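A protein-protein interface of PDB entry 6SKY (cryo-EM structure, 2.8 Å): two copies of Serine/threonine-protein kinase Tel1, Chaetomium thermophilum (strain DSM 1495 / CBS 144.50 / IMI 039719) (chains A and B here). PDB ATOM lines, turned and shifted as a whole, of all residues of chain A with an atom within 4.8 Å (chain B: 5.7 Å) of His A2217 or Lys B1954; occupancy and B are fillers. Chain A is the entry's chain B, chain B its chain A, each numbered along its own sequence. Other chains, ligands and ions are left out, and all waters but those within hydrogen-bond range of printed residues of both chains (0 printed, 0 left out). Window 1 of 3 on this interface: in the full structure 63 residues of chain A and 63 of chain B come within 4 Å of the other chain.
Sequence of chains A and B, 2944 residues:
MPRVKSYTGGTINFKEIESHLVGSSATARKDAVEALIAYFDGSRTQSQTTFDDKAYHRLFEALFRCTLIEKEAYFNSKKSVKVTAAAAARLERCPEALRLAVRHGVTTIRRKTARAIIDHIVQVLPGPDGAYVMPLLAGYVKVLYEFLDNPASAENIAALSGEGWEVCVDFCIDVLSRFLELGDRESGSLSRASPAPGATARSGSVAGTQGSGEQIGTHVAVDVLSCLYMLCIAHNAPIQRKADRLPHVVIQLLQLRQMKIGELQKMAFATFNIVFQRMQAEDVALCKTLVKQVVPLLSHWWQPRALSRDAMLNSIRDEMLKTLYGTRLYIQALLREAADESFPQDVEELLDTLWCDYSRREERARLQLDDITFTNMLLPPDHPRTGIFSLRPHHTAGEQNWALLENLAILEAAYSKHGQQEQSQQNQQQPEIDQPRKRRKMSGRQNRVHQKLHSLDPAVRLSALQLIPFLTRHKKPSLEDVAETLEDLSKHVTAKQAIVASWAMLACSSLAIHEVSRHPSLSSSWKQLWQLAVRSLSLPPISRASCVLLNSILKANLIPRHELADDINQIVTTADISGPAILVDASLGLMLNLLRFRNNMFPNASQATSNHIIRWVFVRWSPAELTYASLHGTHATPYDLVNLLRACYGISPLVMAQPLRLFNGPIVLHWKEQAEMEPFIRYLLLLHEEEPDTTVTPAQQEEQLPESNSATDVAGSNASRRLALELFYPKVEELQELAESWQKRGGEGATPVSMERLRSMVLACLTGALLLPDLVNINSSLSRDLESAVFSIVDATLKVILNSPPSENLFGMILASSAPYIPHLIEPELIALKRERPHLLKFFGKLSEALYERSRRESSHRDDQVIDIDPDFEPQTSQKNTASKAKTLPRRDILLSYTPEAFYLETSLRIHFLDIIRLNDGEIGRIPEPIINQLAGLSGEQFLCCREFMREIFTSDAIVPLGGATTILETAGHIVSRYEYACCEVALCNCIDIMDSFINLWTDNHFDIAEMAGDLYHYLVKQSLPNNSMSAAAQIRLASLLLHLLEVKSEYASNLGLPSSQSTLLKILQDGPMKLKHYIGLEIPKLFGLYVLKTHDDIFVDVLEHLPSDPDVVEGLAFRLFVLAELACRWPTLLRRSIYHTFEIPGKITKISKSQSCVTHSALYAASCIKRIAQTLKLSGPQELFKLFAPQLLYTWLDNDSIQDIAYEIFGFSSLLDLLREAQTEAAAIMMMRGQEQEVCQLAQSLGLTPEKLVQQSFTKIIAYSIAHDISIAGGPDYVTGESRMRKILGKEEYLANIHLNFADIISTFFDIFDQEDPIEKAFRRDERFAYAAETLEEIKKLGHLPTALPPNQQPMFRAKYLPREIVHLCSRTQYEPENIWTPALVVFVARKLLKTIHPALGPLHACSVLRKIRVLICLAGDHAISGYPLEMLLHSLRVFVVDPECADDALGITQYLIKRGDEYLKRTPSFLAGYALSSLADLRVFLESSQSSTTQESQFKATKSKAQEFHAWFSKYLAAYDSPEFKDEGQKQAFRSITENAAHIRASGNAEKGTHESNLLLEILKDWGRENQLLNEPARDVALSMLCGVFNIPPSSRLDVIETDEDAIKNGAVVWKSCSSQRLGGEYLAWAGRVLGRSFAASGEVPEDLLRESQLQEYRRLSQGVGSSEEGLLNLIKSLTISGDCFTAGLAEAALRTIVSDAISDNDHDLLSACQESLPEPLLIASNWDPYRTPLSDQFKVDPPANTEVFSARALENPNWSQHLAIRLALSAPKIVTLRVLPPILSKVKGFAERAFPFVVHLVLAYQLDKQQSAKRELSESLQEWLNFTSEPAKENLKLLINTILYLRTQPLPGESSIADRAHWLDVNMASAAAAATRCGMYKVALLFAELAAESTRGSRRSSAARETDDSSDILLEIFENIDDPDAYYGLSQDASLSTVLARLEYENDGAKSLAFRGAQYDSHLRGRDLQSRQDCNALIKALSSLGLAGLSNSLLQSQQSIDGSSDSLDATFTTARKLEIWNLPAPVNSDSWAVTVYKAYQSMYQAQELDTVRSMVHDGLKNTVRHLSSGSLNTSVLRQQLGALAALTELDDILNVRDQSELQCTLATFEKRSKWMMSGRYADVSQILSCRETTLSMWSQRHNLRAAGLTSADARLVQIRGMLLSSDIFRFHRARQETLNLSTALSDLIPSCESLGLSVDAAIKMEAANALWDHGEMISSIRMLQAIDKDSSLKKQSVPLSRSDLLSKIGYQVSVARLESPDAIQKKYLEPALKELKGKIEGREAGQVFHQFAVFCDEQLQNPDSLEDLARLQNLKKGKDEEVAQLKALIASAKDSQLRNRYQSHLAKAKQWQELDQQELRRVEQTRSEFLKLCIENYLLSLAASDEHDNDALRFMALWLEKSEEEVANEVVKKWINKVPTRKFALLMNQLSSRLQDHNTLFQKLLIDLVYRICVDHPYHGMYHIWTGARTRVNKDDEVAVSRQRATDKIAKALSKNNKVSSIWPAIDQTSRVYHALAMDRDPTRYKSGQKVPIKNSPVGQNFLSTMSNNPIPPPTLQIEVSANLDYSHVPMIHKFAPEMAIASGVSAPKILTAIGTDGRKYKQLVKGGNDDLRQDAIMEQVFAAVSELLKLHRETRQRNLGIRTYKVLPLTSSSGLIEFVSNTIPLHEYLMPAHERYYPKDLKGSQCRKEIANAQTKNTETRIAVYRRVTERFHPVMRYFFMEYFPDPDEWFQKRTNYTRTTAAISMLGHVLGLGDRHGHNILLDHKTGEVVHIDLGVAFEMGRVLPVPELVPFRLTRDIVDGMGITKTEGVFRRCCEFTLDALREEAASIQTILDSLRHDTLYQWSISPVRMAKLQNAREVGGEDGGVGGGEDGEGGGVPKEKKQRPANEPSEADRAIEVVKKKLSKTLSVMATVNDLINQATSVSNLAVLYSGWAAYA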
ATOM      1  N   ARG A2178      -5.397  18.226  22.675  1.00  0.00           N
ATOM      2  CA  ARG A2178      -4.099  18.781  22.312  1.00  0.00           C
ATOM      3  C   ARG A2178      -3.951  20.207  22.810  1.00  0.00           C
ATOM      4  O   ARG A2178      -2.907  20.581  23.358  1.00  0.00           O
ATOM      5  CB  ARG A2178      -3.909  18.742  20.799  1.00  0.00           C
ATOM      6  CG  ARG A2178      -4.038  17.391  20.166  1.00  0.00           C
ATOM      7  CD  ARG A2178      -3.207  16.373  20.881  1.00  0.00           C
ATOM      8  NE  ARG A2178      -3.290  15.074  20.226  1.00  0.00           N
ATOM      9  CZ  ARG A2178      -3.026  13.920  20.826  1.00  0.00           C
ATOM     10  NH1 ARG A2178      -3.122  12.787  20.151  1.00  0.00           N
ATOM     11  NH2 ARG A2178      -2.679  13.899  22.104  1.00  0.00           N
ATOM     12  N   THR A2181      -3.199  20.499  26.643  1.00  0.00           N
ATOM     13  CA  THR A2181      -1.821  20.192  27.007  1.00  0.00           C
ATOM     14  C   THR A2181      -0.881  21.293  26.551  1.00  0.00           C
ATOM     15  O   THR A2181       0.080  21.622  27.249  1.00  0.00           O
ATOM     16  CB  THR A2181      -1.389  18.859  26.412  1.00  0.00           C
ATOM     17  OG1 THR A2181      -1.422  18.944  24.987  1.00  0.00           O
ATOM     18  CG2 THR A2181      -2.299  17.763  26.859  1.00  0.00           C
ATOM     19  N   LEU A2182      -1.149  21.882  25.388  1.00  0.00           N
ATOM     20  CA  LEU A2182      -0.348  23.007  24.921  1.00  0.00           C
ATOM     21  C   LEU A2182      -0.463  24.196  25.865  1.00  0.00           C
ATOM     22  O   LEU A2182       0.545  24.792  26.259  1.00  0.00           O
ATOM     23  CB  LEU A2182      -0.795  23.383  23.516  1.00  0.00           C
ATOM     24  CG  LEU A2182       0.192  23.998  22.549  1.00  0.00           C
ATOM     25  CD1 LEU A2182       1.495  23.273  22.644  1.00  0.00           C
ATOM     26  CD2 LEU A2182      -0.377  23.856  21.184  1.00  0.00           C
ATOM     27  N   ALA A2213       4.304  17.597  25.103  1.00  0.00           N
ATOM     28  CA  ALA A2213       3.389  18.343  24.248  1.00  0.00           C
ATOM     29  C   ALA A2213       3.849  18.323  22.796  1.00  0.00           C
ATOM     30  O   ALA A2213       3.057  18.066  21.881  1.00  0.00           O
ATOM     31  CB  ALA A2213       3.257  19.772  24.755  1.00  0.00           C
ATOM     32  N   LEU A2214       5.139  18.581  22.566  1.00  0.00           N
ATOM     33  CA  LEU A2214       5.681  18.514  21.210  1.00  0.00           C
ATOM     34  C   LEU A2214       5.448  17.147  20.585  1.00  0.00           C
ATOM     35  O   LEU A2214       4.972  17.046  19.455  1.00  0.00           O
ATOM     36  CB  LEU A2214       7.168  18.841  21.213  1.00  0.00           C
ATOM     37  CG  LEU A2214       7.531  20.310  21.346  1.00  0.00           C
ATOM     38  CD1 LEU A2214       9.022  20.483  21.344  1.00  0.00           C
ATOM     39  CD2 LEU A2214       6.904  21.082  20.235  1.00  0.00           C
ATOM     40  N   TRP A2215       5.783  16.081  21.305  1.00  0.00           N
ATOM     41  CA  TRP A2215       5.617  14.743  20.756  1.00  0.00           C
ATOM     42  C   TRP A2215       4.169  14.453  20.424  1.00  0.00           C
ATOM     43  O   TRP A2215       3.880  13.760  19.446  1.00  0.00           O
ATOM     44  CB  TRP A2215       6.139  13.697  21.731  1.00  0.00           C
ATOM     45  CG  TRP A2215       5.956  12.298  21.256  1.00  0.00           C
ATOM     46  CD1 TRP A2215       4.928  11.470  21.550  1.00  0.00           C
ATOM     47  CD2 TRP A2215       6.833  11.560  20.404  1.00  0.00           C
ATOM     48  NE1 TRP A2215       5.102  10.262  20.939  1.00  0.00           N
ATOM     49  CE2 TRP A2215       6.267  10.293  20.224  1.00  0.00           C
ATOM     50  CE3 TRP A2215       8.043  11.848  19.774  1.00  0.00           C
ATOM     51  CZ2 TRP A2215       6.865   9.321  19.448  1.00  0.00           C
ATOM     52  CZ3 TRP A2215       8.629  10.884  19.007  1.00  0.00           C
ATOM     53  CH2 TRP A2215       8.044   9.637  18.849  1.00  0.00           C
ATOM     54  N   ASP A2216       3.241  14.957  21.224  1.00  0.00           N
ATOM     55  CA  ASP A2216       1.840  14.682  20.946  1.00  0.00           C
ATOM     56  C   ASP A2216       1.258  15.573  19.864  1.00  0.00           C
ATOM     57  O   ASP A2216       0.156  15.298  19.391  1.00  0.00           O
ATOM     58  CB  ASP A2216       1.022  14.793  22.227  1.00  0.00           C
ATOM     59  CG  ASP A2216       1.207  13.587  23.127  1.00  0.00           C
ATOM     60  OD1 ASP A2216       2.093  13.616  24.003  1.00  0.00           O
ATOM     61  OD2 ASP A2216       0.485  12.588  22.939  1.00  0.00           O
ATOM     62  N   HIS A2217       1.959  16.618  19.450  1.00  0.00           N
ATOM     63  CA  HIS A2217       1.534  17.364  18.274  1.00  0.00           C
ATOM     64  C   HIS A2217       2.185  16.895  16.984  1.00  0.00           C
ATOM     65  O   HIS A2217       1.879  17.447  15.926  1.00  0.00           O
ATOM     66  CB  HIS A2217       1.801  18.848  18.459  1.00  0.00           C
ATOM     67  CG  HIS A2217       0.678  19.567  19.124  1.00  0.00           C
ATOM     68  ND1 HIS A2217       0.546  19.636  20.490  1.00  0.00           N
ATOM     69  CD2 HIS A2217      -0.385  20.223  18.608  1.00  0.00           C
ATOM     70  CE1 HIS A2217      -0.540  20.318  20.790  1.00  0.00           C
ATOM     71  NE2 HIS A2217      -1.124  20.686  19.666  1.00  0.00           N
ATOM     72  N   GLY A2218       3.071  15.909  17.033  1.00  0.00           N
ATOM     73  CA  GLY A2218       3.689  15.387  15.837  1.00  0.00           C
ATOM     74  C   GLY A2218       5.121  15.808  15.595  1.00  0.00           C
ATOM     75  O   GLY A2218       5.726  15.330  14.634  1.00  0.00           O
ATOM     76  N   GLU A2219       5.682  16.682  16.424  1.00  0.00           N
ATOM     77  CA  GLU A2219       7.073  17.105  16.275  1.00  0.00           C
ATOM     78  C   GLU A2219       7.963  16.092  16.972  1.00  0.00           C
ATOM     79  O   GLU A2219       8.271  16.216  18.151  1.00  0.00           O
ATOM     80  CB  GLU A2219       7.284  18.492  16.853  1.00  0.00           C
ATOM     81  CG  GLU A2219       6.145  19.440  16.632  1.00  0.00           C
ATOM     82  CD  GLU A2219       5.901  19.715  15.179  1.00  0.00           C
ATOM     83  OE1 GLU A2219       4.768  19.491  14.719  1.00  0.00           O
ATOM     84  OE2 GLU A2219       6.844  20.151  14.488  1.00  0.00           O
ATOM     85  N   LEU B1943       7.512  27.109  17.037  1.00  0.00           N
ATOM     86  CA  LEU B1943       6.629  28.174  16.579  1.00  0.00           C
ATOM     87  C   LEU B1943       7.306  29.042  15.526  1.00  0.00           C
ATOM     88  O   LEU B1943       6.671  29.455  14.552  1.00  0.00           O
ATOM     89  CB  LEU B1943       6.180  29.014  17.771  1.00  0.00           C
ATOM     90  CG  LEU B1943       5.175  30.126  17.514  1.00  0.00           C
ATOM     91  CD1 LEU B1943       4.031  29.626  16.665  1.00  0.00           C
ATOM     92  CD2 LEU B1943       4.682  30.638  18.837  1.00  0.00           C
ATOM     93  N   LEU B1946       7.153  27.191  12.354  1.00  0.00           N
ATOM     94  CA  LEU B1946       5.807  27.145  11.790  1.00  0.00           C
ATOM     95  C   LEU B1946       5.388  28.484  11.214  1.00  0.00           C
ATOM     96  O   LEU B1946       4.586  28.529  10.280  1.00  0.00           O
ATOM     97  CB  LEU B1946       4.802  26.705  12.847  1.00  0.00           C
ATOM     98  CG  LEU B1946       4.793  25.233  13.222  1.00  0.00           C
ATOM     99  CD1 LEU B1946       3.951  25.045  14.448  1.00  0.00           C
ATOM    100  CD2 LEU B1946       4.253  24.422  12.075  1.00  0.00           C
ATOM    101  N   ASP B1951       2.321  28.166   8.287  1.00  0.00           N
ATOM    102  CA  ASP B1951       1.309  27.162   8.552  1.00  0.00           C
ATOM    103  C   ASP B1951       0.021  27.834   9.014  1.00  0.00           C
ATOM    104  O   ASP B1951      -0.008  29.006   9.392  1.00  0.00           O
ATOM    105  CB  ASP B1951       1.802  26.158   9.587  1.00  0.00           C
ATOM    106  CG  ASP B1951       1.060  24.843   9.515  1.00  0.00           C
ATOM    107  OD1 ASP B1951      -0.103  24.837   9.066  1.00  0.00           O
ATOM    108  OD2 ASP B1951       1.638  23.810   9.907  1.00  0.00           O
ATOM    109  N   GLY B1952      -1.057  27.067   8.997  1.00  0.00           N
ATOM    110  CA  GLY B1952      -2.369  27.636   9.213  1.00  0.00           C
ATOM    111  C   GLY B1952      -2.799  27.558  10.655  1.00  0.00           C
ATOM    112  O   GLY B1952      -2.373  28.371  11.476  1.00  0.00           O
ATOM    113  N   ALA B1953      -3.668  26.599  10.968  1.00  0.00           N
ATOM    114  CA  ALA B1953      -4.093  26.408  12.344  1.00  0.00           C
ATOM    115  C   ALA B1953      -2.966  25.924  13.238  1.00  0.00           C
ATOM    116  O   ALA B1953      -3.041  26.093  14.461  1.00  0.00           O
ATOM    117  CB  ALA B1953      -5.255  25.419  12.396  1.00  0.00           C
ATOM    118  N   LYS B1954      -1.923  25.334  12.662  1.00  0.00           N
ATOM    119  CA  LYS B1954      -0.869  24.756  13.482  1.00  0.00           C
ATOM    120  C   LYS B1954      -0.071  25.834  14.194  1.00  0.00           C
ATOM    121  O   LYS B1954       0.372  25.634  15.328  1.00  0.00           O
ATOM    122  CB  LYS B1954       0.040  23.891  12.621  1.00  0.00           C
ATOM    123  CG  LYS B1954       1.119  23.175  13.387  1.00  0.00           C
ATOM    124  CD  LYS B1954       0.697  21.785  13.791  1.00  0.00           C
ATOM    125  CE  LYS B1954       1.870  21.012  14.353  1.00  0.00           C
ATOM    126  NZ  LYS B1954       1.489  19.610  14.664  1.00  0.00           N
ATOM    127  N   SER B1955       0.135  26.978  13.554  1.00  0.00           N
ATOM    128  CA  SER B1955       0.774  28.077  14.259  1.00  0.00           C
ATOM    129  C   SER B1955      -0.217  28.859  15.093  1.00  0.00           C
ATOM    130  O   SER B1955       0.181  29.484  16.076  1.00  0.00           O
ATOM    131  CB  SER B1955       1.480  29.010  13.279  1.00  0.00           C
ATOM    132  OG  SER B1955       0.568  29.589  12.375  1.00  0.00           O
ATOM    133  N   LEU B1956      -1.497  28.822  14.729  1.00  0.00           N
ATOM    134  CA  LEU B1956      -2.519  29.480  15.530  1.00  0.00           C
ATOM    135  C   LEU B1956      -2.635  28.842  16.903  1.00  0.00           C
ATOM    136  O   LEU B1956      -2.848  29.539  17.894  1.00  0.00           O
ATOM    137  CB  LEU B1956      -3.857  29.437  14.801  1.00  0.00           C
ATOM    138  CG  LEU B1956      -5.096  29.863  15.574  1.00  0.00           C
ATOM    139  CD1 LEU B1956      -4.973  31.287  16.026  1.00  0.00           C
ATOM    140  CD2 LEU B1956      -6.314  29.701  14.711  1.00  0.00           C
ATOM    141  N   ALA B1957      -2.454  27.525  16.991  1.00  0.00           N
ATOM    142  CA  ALA B1957      -2.483  26.849  18.284  1.00  0.00           C
ATOM    143  C   ALA B1957      -1.368  27.340  19.203  1.00  0.00           C
ATOM    144  O   ALA B1957      -1.618  27.785  20.330  1.00  0.00           O
ATOM    145  CB  ALA B1957      -2.374  25.344  18.076  1.00  0.00           C
ATOM    146  N   PHE B1958      -0.124  27.252  18.736  1.00  0.00           N
ATOM    147  CA  PHE B1958       1.017  27.643  19.553  1.00  0.00           C
ATOM    148  C   PHE B1958       0.995  29.132  19.869  1.00  0.00           C
ATOM    149  O   PHE B1958       1.341  29.545  20.983  1.00  0.00           O
ATOM    150  CB  PHE B1958       2.314  27.270  18.845  1.00  0.00           C
ATOM    151  CG  PHE B1958       2.573  25.800  18.779  1.00  0.00           C
ATOM    152  CD1 PHE B1958       1.904  25.005  17.882  1.00  0.00           C
ATOM    153  CD2 PHE B1958       3.494  25.212  19.610  1.00  0.00           C
ATOM    154  CE1 PHE B1958       2.141  23.660  17.827  1.00  0.00           C
ATOM    155  CE2 PHE B1958       3.731  23.869  19.548  1.00  0.00           C
ATOM    156  CZ  PHE B1958       3.054  23.095  18.658  1.00  0.00           C
ATOM    157  N   ARG B1959       0.576  29.956  18.908  1.00  0.00           N
ATOM    158  CA  ARG B1959       0.501  31.388  19.151  1.00  0.00           C
ATOM    159  C   ARG B1959      -0.601  31.733  20.135  1.00  0.00           C
ATOM    160  O   ARG B1959      -0.418  32.611  20.976  1.00  0.00           O
ATOM    161  CB  ARG B1959       0.284  32.135  17.847  1.00  0.00           C
ATOM    162  CG  ARG B1959       1.530  32.687  17.250  1.00  0.00           C
ATOM    163  CD  ARG B1959       2.319  33.480  18.250  1.00  0.00           C
ATOM    164  NE  ARG B1959       3.660  33.724  17.745  1.00  0.00           N
ATOM    165  CZ  ARG B1959       4.621  34.314  18.438  1.00  0.00           C
ATOM    166  NH1 ARG B1959       5.813  34.492  17.896  1.00  0.00           N
ATOM    167  NH2 ARG B1959       4.389  34.721  19.673  1.00  0.00           N
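NZ of Lys B1954 is in hydrogen-bond range of O of His A2217, 2.5 Å away.
NZ of Lys B1954 is in salt-bridge range of OE1 of Glu A2219.
No position is printed for both chains.
Of the 4 pairs that touch across the chains among the printed residues, none has its exchanged pair printed and touching as well.
Thr A2181 touches none of the printed residues of chain B.
Of the printed residues of chain B, Leu A2182 touches Ala B1957 (3.98 Å) and Phe B1958 (3.9 Å).
His A2217 touches one residue of chain B.
Of the printed residues of chain B, Glu A2219 touches Lys B1954.
Lys B1954 touches two residues of chain A.
Printed residues of chain A within 4 Å of Ala B1957: Leu A2182 (3.98 Å).
Of the printed residues of chain A, Phe B1958 touches Leu A2182.
The nearest residue of chain A that does not touch Lys B1954 is Gly A2218 (4.7 Å).
ND1 of His A2217 sits at hydrogen-bond distance from O of Ala A2213 (3.3 Å).
The backbone carbonyl oxygen (O) of Leu A2214 sits at hydrogen-bond distance from the backbone NH (N) of Glu A2219 (3.1 Å).
Leu A2182 touches Ala B1957 (CD2 to CB, 3.98 Å).
Phe B1958 touches Leu A2182.
Hydrophobic or aromatic side chains of chain B within 4 Å of the printed part of chain A: Ala B1957 and Phe B1958.
Along chain B the printed residues that touch a printed residue of chain A span positions 1954 to 1958.
Printed residues of chain A that touch a printed residue of chain B: Leu A2182, His A2217 and Glu A2219.
Hydrophobic or aromatic side chains of chain A that line the printed part of chain B: Leu A2182 and His A2217.
Among the printed residues, 4 pairs touch across the chains.
Among the printed residues, Asp or Glu carboxylates within 4 Å of a Lys or Arg side-chain nitrogen of the other chain: Glu A2219 with Lys B1954 (3.3 Å).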
